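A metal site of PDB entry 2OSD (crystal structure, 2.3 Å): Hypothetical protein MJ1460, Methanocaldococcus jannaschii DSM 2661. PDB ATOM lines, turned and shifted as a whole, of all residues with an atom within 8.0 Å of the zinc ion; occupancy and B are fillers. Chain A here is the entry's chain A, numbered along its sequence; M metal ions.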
ATOM      1  N   LEU A 102       4.420  35.261   4.079  1.00  0.00           N
ATOM      2  CA  LEU A 102       4.439  35.808   2.754  1.00  0.00           C
ATOM      3  C   LEU A 102       3.033  36.317   2.467  1.00  0.00           C
ATOM      4  O   LEU A 102       2.081  35.547   2.481  1.00  0.00           O
ATOM      5  CB  LEU A 102       4.857  34.757   1.714  1.00  0.00           C
ATOM      6  CG  LEU A 102       4.939  35.201   0.243  1.00  0.00           C
ATOM      7  CD1 LEU A 102       5.871  36.381  -0.003  1.00  0.00           C
ATOM      8  CD2 LEU A 102       5.354  34.039  -0.605  1.00  0.00           C
ATOM      9  N   PRO A 105       1.111  36.525  -2.233  1.00  0.00           N
ATOM     10  CA  PRO A 105       1.970  35.650  -3.017  1.00  0.00           C
ATOM     11  C   PRO A 105       1.355  35.359  -4.375  1.00  0.00           C
ATOM     12  O   PRO A 105       0.264  35.769  -4.625  1.00  0.00           O
ATOM     13  CB  PRO A 105       1.981  34.390  -2.170  1.00  0.00           C
ATOM     14  CG  PRO A 105       0.597  34.351  -1.603  1.00  0.00           C
ATOM     15  CD  PRO A 105       0.255  35.752  -1.301  1.00  0.00           C
ATOM     16  N   PRO A 106       2.060  34.642  -5.255  1.00  0.00           N
ATOM     17  CA  PRO A 106       1.469  34.211  -6.546  1.00  0.00           C
ATOM     18  C   PRO A 106       0.407  33.156  -6.335  1.00  0.00           C
ATOM     19  O   PRO A 106       0.366  32.563  -5.275  1.00  0.00           O
ATOM     20  CB  PRO A 106       2.662  33.605  -7.313  1.00  0.00           C
ATOM     21  CG  PRO A 106       3.828  34.043  -6.610  1.00  0.00           C
ATOM     22  CD  PRO A 106       3.442  34.227  -5.159  1.00  0.00           C
ATOM     23  N   TYR A 107      -0.461  32.963  -7.335  1.00  0.00           N
ATOM     24  CA  TYR A 107      -1.564  31.986  -7.286  1.00  0.00           C
ATOM     25  C   TYR A 107      -2.579  32.214  -6.180  1.00  0.00           C
ATOM     26  O   TYR A 107      -3.137  31.280  -5.654  1.00  0.00           O
ATOM     27  CB  TYR A 107      -1.029  30.562  -7.200  1.00  0.00           C
ATOM     28  CG  TYR A 107      -0.036  30.223  -8.271  1.00  0.00           C
ATOM     29  CD1 TYR A 107      -0.401  30.267  -9.613  1.00  0.00           C
ATOM     30  CD2 TYR A 107       1.263  29.837  -7.944  1.00  0.00           C
ATOM     31  CE1 TYR A 107       0.513  29.961 -10.610  1.00  0.00           C
ATOM     32  CE2 TYR A 107       2.181  29.508  -8.918  1.00  0.00           C
ATOM     33  CZ  TYR A 107       1.793  29.558 -10.254  1.00  0.00           C
ATOM     34  OH  TYR A 107       2.680  29.241 -11.242  1.00  0.00           O
ATOM     35  N   GLU A 114      -4.222  21.451   0.685  1.00  0.00           N
ATOM     36  CA  GLU A 114      -2.831  21.529   1.127  1.00  0.00           C
ATOM     37  C   GLU A 114      -2.105  22.728   0.483  1.00  0.00           C
ATOM     38  O   GLU A 114      -2.472  23.160  -0.608  1.00  0.00           O
ATOM     39  CB  GLU A 114      -2.097  20.197   0.903  1.00  0.00           C
ATOM     40  CG  GLU A 114      -2.556  19.039   1.863  1.00  0.00           C
ATOM     41  CD  GLU A 114      -2.275  19.295   3.368  1.00  0.00           C
ATOM     42  N   PRO A 115      -1.102  23.283   1.184  1.00  0.00           N
ATOM     43  CA  PRO A 115      -0.336  24.406   0.673  1.00  0.00           C
ATOM     44  C   PRO A 115       0.277  24.125  -0.693  1.00  0.00           C
ATOM     45  O   PRO A 115       0.653  22.988  -0.969  1.00  0.00           O
ATOM     46  CB  PRO A 115       0.751  24.570   1.720  1.00  0.00           C
ATOM     47  CG  PRO A 115       0.165  24.039   2.955  1.00  0.00           C
ATOM     48  CD  PRO A 115      -0.662  22.910   2.545  1.00  0.00           C
ATOM     49  N   ILE A 116       0.364  25.157  -1.534  1.00  0.00           N
ATOM     50  CA  ILE A 116       0.776  25.017  -2.914  1.00  0.00           C
ATOM     51  C   ILE A 116       2.135  25.624  -3.211  1.00  0.00           C
ATOM     52  O   ILE A 116       2.680  25.365  -4.270  1.00  0.00           O
ATOM     53  CB  ILE A 116      -0.254  25.651  -3.906  1.00  0.00           C
ATOM     54  CG1 ILE A 116      -0.374  27.171  -3.745  1.00  0.00           C
ATOM     55  CG2 ILE A 116      -1.631  24.963  -3.770  1.00  0.00           C
ATOM     56  CD1 ILE A 116      -1.181  27.879  -4.860  1.00  0.00           C
ATOM     57  N   HIS A 117       2.707  26.421  -2.306  1.00  0.00           N
ATOM     58  CA  HIS A 117       3.989  27.120  -2.614  1.00  0.00           C
ATOM     59  C   HIS A 117       5.287  26.370  -2.340  1.00  0.00           C
ATOM     60  O   HIS A 117       6.178  26.852  -1.660  1.00  0.00           O
ATOM     61  CB  HIS A 117       3.975  28.509  -1.981  1.00  0.00           C
ATOM     62  CG  HIS A 117       2.950  29.426  -2.592  1.00  0.00           C
ATOM     63  ND1 HIS A 117       1.796  29.795  -1.941  1.00  0.00           N
ATOM     64  CD2 HIS A 117       2.880  29.992  -3.817  1.00  0.00           C
ATOM     65  CE1 HIS A 117       1.087  30.596  -2.706  1.00  0.00           C
ATOM     66  NE2 HIS A 117       1.721  30.722  -3.866  1.00  0.00           N
ATOM     67  N   ASP A 118       5.409  25.180  -2.906  1.00  0.00           N
ATOM     68  CA  ASP A 118       6.587  24.374  -2.725  1.00  0.00           C
ATOM     69  C   ASP A 118       7.823  25.003  -3.333  1.00  0.00           C
ATOM     70  O   ASP A 118       8.912  24.960  -2.756  1.00  0.00           O
ATOM     71  CB  ASP A 118       6.403  23.006  -3.381  1.00  0.00           C
ATOM     72  CG  ASP A 118       5.451  22.130  -2.636  1.00  0.00           C
ATOM     73  OD1 ASP A 118       4.708  22.657  -1.770  1.00  0.00           O
ATOM     74  OD2 ASP A 118       5.432  20.930  -2.952  1.00  0.00           O
ATOM     75  N   ILE A 120       8.456  28.294  -4.005  1.00  0.00           N
ATOM     76  CA  ILE A 120       8.827  29.369  -3.078  1.00  0.00           C
ATOM     77  C   ILE A 120       9.496  28.876  -1.763  1.00  0.00           C
ATOM     78  O   ILE A 120      10.433  29.503  -1.276  1.00  0.00           O
ATOM     79  CB  ILE A 120       7.611  30.314  -2.782  1.00  0.00           C
ATOM     80  CG1 ILE A 120       7.360  31.277  -3.946  1.00  0.00           C
ATOM     81  CG2 ILE A 120       7.789  31.153  -1.502  1.00  0.00           C
ATOM     82  CD1 ILE A 120       6.021  32.085  -3.820  1.00  0.00           C
ATOM     83  N   GLU A 140       6.166  24.820   4.276  1.00  0.00           N
ATOM     84  CA  GLU A 140       4.972  25.647   4.284  1.00  0.00           C
ATOM     85  C   GLU A 140       3.886  24.966   5.079  1.00  0.00           C
ATOM     86  O   GLU A 140       3.492  23.854   4.731  1.00  0.00           O
ATOM     87  CB  GLU A 140       4.489  25.931   2.852  1.00  0.00           C
ATOM     88  CG  GLU A 140       3.483  27.041   2.824  1.00  0.00           C
ATOM     89  CD  GLU A 140       2.952  27.348   1.449  1.00  0.00           C
ATOM     90  OE1 GLU A 140       2.927  26.454   0.570  1.00  0.00           O
ATOM     91  OE2 GLU A 140       2.552  28.488   1.273  1.00  0.00           O
ATOM     92  N   VAL A 141       3.426  25.624   6.148  1.00  0.00           N
ATOM     93  CA  VAL A 141       2.453  25.042   7.067  1.00  0.00           C
ATOM     94  C   VAL A 141       1.051  25.691   7.007  1.00  0.00           C
ATOM     95  O   VAL A 141       0.082  25.143   7.530  1.00  0.00           O
ATOM     96  CB  VAL A 141       3.018  25.025   8.540  1.00  0.00           C
ATOM     97  CG1 VAL A 141       4.091  23.966   8.663  1.00  0.00           C
ATOM     98  CG2 VAL A 141       3.557  26.402   8.977  1.00  0.00           C
ATOM     99  N   GLU A 142       0.949  26.863   6.392  1.00  0.00           N
ATOM    100  CA  GLU A 142      -0.342  27.511   6.077  1.00  0.00           C
ATOM    101  C   GLU A 142      -0.166  28.145   4.722  1.00  0.00           C
ATOM    102  O   GLU A 142       0.931  28.481   4.387  1.00  0.00           O
ATOM    103  CB  GLU A 142      -0.712  28.589   7.094  1.00  0.00           C
ATOM    104  CG  GLU A 142      -0.907  28.104   8.513  1.00  0.00           C
ATOM    105  CD  GLU A 142      -1.580  29.139   9.379  1.00  0.00           C
ATOM    106  OE1 GLU A 142      -1.522  30.342   9.055  1.00  0.00           O
ATOM    107  OE2 GLU A 142      -2.169  28.756  10.415  1.00  0.00           O
ATOM    108  N   CYS A 143      -1.248  28.315   3.980  1.00  0.00           N
ATOM    109  CA  CYS A 143      -1.219  28.844   2.631  1.00  0.00           C
ATOM    110  C   CYS A 143      -2.457  29.657   2.343  1.00  0.00           C
ATOM    111  O   CYS A 143      -3.543  29.318   2.778  1.00  0.00           O
ATOM    112  CB  CYS A 143      -1.114  27.689   1.640  1.00  0.00           C
ATOM    113  SG  CYS A 143      -0.719  28.128  -0.095  1.00  0.00           S
ATOM    114  N   VAL A 144      -2.285  30.759   1.649  1.00  0.00           N
ATOM    115  CA  VAL A 144      -3.398  31.505   1.031  1.00  0.00           C
ATOM    116  C   VAL A 144      -4.383  30.580   0.257  1.00  0.00           C
ATOM    117  O   VAL A 144      -5.575  30.821   0.247  1.00  0.00           O
ATOM    118  CB  VAL A 144      -2.827  32.686   0.168  1.00  0.00           C
ATOM    119  CG1 VAL A 144      -3.874  33.318  -0.670  1.00  0.00           C
ATOM    120  CG2 VAL A 144      -2.248  33.745   1.086  1.00  0.00           C
ATOM    121  N   SER A 145      -3.877  29.490  -0.319  1.00  0.00           N
ATOM    122  CA  SER A 145      -4.688  28.452  -0.983  1.00  0.00           C
ATOM    123  C   SER A 145      -5.790  27.867  -0.114  1.00  0.00           C
ATOM    124  O   SER A 145      -6.771  27.301  -0.622  1.00  0.00           O
ATOM    125  CB  SER A 145      -3.806  27.298  -1.536  1.00  0.00           C
ATOM    126  OG  SER A 145      -3.624  26.215  -0.595  1.00  0.00           O
ATOM    127  N   GLN A 146      -5.630  27.972   1.207  1.00  0.00           N
ATOM    128  CA  GLN A 146      -6.594  27.445   2.157  1.00  0.00           C
ATOM    129  C   GLN A 146      -7.525  28.526   2.706  1.00  0.00           C
ATOM    130  O   GLN A 146      -8.280  28.267   3.637  1.00  0.00           O
ATOM    131  CB  GLN A 146      -5.846  26.796   3.308  1.00  0.00           C
ATOM    132  CG  GLN A 146      -4.824  25.797   2.867  1.00  0.00           C
ATOM    133  CD  GLN A 146      -3.851  25.409   3.965  1.00  0.00           C
ATOM    134  OE1 GLN A 146      -3.459  26.270   4.780  1.00  0.00           O
ATOM    135  NE2 GLN A 146      -3.446  24.098   3.972  1.00  0.00           N
ATOM    136  N   LYS A 148      -6.372  31.410   3.980  1.00  0.00           N
ATOM    137  CA  LYS A 148      -5.608  32.165   4.971  1.00  0.00           C
ATOM    138  C   LYS A 148      -5.186  33.492   4.359  1.00  0.00           C
ATOM    139  O   LYS A 148      -5.111  33.626   3.160  1.00  0.00           O
ATOM    140  CB  LYS A 148      -4.367  31.389   5.419  1.00  0.00           C
ATOM    141  CG  LYS A 148      -4.600  29.997   5.970  1.00  0.00           C
ATOM    142  CD  LYS A 148      -5.591  30.029   7.073  1.00  0.00           C
ATOM    143  CE  LYS A 148      -5.428  28.892   8.022  1.00  0.00           C
ATOM    144  NZ  LYS A 148      -6.227  29.207   9.243  1.00  0.00           N
ATOM    145  N   LYS A 150      -2.152  34.913   4.901  1.00  0.00           N
ATOM    146  CA  LYS A 150      -0.760  34.815   4.495  1.00  0.00           C
ATOM    147  C   LYS A 150      -0.292  33.374   4.424  1.00  0.00           C
ATOM    148  O   LYS A 150      -0.848  32.496   5.064  1.00  0.00           O
ATOM    149  CB  LYS A 150       0.152  35.584   5.470  1.00  0.00           C
ATOM    150  CG  LYS A 150      -0.393  36.924   5.940  1.00  0.00           C
ATOM    151  CD  LYS A 150       0.622  37.690   6.773  1.00  0.00           C
ATOM    152  CE  LYS A 150       0.011  38.949   7.386  1.00  0.00           C
ATOM    153  NZ  LYS A 150       0.905  39.634   8.371  1.00  0.00           N
ATOM    154  N   CYS A 151       0.728  33.145   3.613  1.00  0.00           N
ATOM    155  CA  CYS A 151       1.451  31.899   3.638  1.00  0.00           C
ATOM    156  C   CYS A 151       2.430  31.936   4.814  1.00  0.00           C
ATOM    157  O   CYS A 151       3.093  32.941   5.050  1.00  0.00           O
ATOM    158  CB  CYS A 151       2.180  31.677   2.323  1.00  0.00           C
ATOM    159  SG  CYS A 151       1.009  31.306   0.996  1.00  0.00           S
ATOM    160  N   VAL A 152       2.502  30.835   5.566  1.00  0.00           N
ATOM    161  CA  VAL A 152       3.399  30.742   6.707  1.00  0.00           C
ATOM    162  C   VAL A 152       4.323  29.537   6.499  1.00  0.00           C
ATOM    163  O   VAL A 152       3.865  28.427   6.200  1.00  0.00           O
ATOM    164  CB  VAL A 152       2.635  30.638   8.016  1.00  0.00           C
ATOM    165  CG1 VAL A 152       3.601  30.487   9.191  1.00  0.00           C
ATOM    166  CG2 VAL A 152       1.755  31.864   8.179  1.00  0.00           C
ATOM    167  N   PHE A 153       5.628  29.791   6.625  1.00  0.00           N
ATOM    168  CA  PHE A 153       6.679  28.833   6.327  1.00  0.00           C
ATOM    169  C   PHE A 153       7.498  28.650   7.563  1.00  0.00           C
ATOM    170  O   PHE A 153       8.008  29.631   8.062  1.00  0.00           O
ATOM    171  CB  PHE A 153       7.603  29.411   5.283  1.00  0.00           C
ATOM    172  CG  PHE A 153       6.960  29.694   3.951  1.00  0.00           C
ATOM    173  CD1 PHE A 153       6.952  28.723   2.953  1.00  0.00           C
ATOM    174  CD2 PHE A 153       6.407  30.916   3.684  1.00  0.00           C
ATOM    175  CE1 PHE A 153       6.380  28.967   1.720  1.00  0.00           C
ATOM    176  CE2 PHE A 153       5.826  31.172   2.438  1.00  0.00           C
ATOM    177  CZ  PHE A 153       5.817  30.192   1.463  1.00  0.00           C
HETATM  178 ZN    ZN M   1       1.206  29.511   0.088  1.00  0.00          ZN
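SG of Cys 151 lies close to N of Val 144, 3.4 Å away.
The backbone NH (N) of Leu 102 lies within hydrogen-bond range of the backbone carbonyl oxygen (O) of Cys 151, 2.8 Å away.
The backbone carbonyl oxygen (O) of Pro 106 lies within hydrogen-bond range of a ring nitrogen (NE2) of His 117, at 2.7 Å.
The side-chain sulfur (SG) of Cys 143 lies close to the backbone NH (N) of Ile 116 (3.5 Å).
N of Ser 145 sits close to SG of Cys 143 (3.4 Å).
The backbone NH (N) of Cys 143 lies within hydrogen-bond range of the side-chain amide oxygen (OE1) of Gln 146 (3.1 Å).
Within 4 Å of the zinc ion: His 117, Glu 140, Cys 143 and Cys 151.
The nearest printed residue that does not touch the zinc ion is Val 144 (4.02 Å).
The zinc ion is bound by SG of Cys 151 (2.0 Å), OE2 of Glu 140 (2.1 Å), ND1 of His 117 (2.1 Å) and SG of Cys 143 (2.4 Å).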
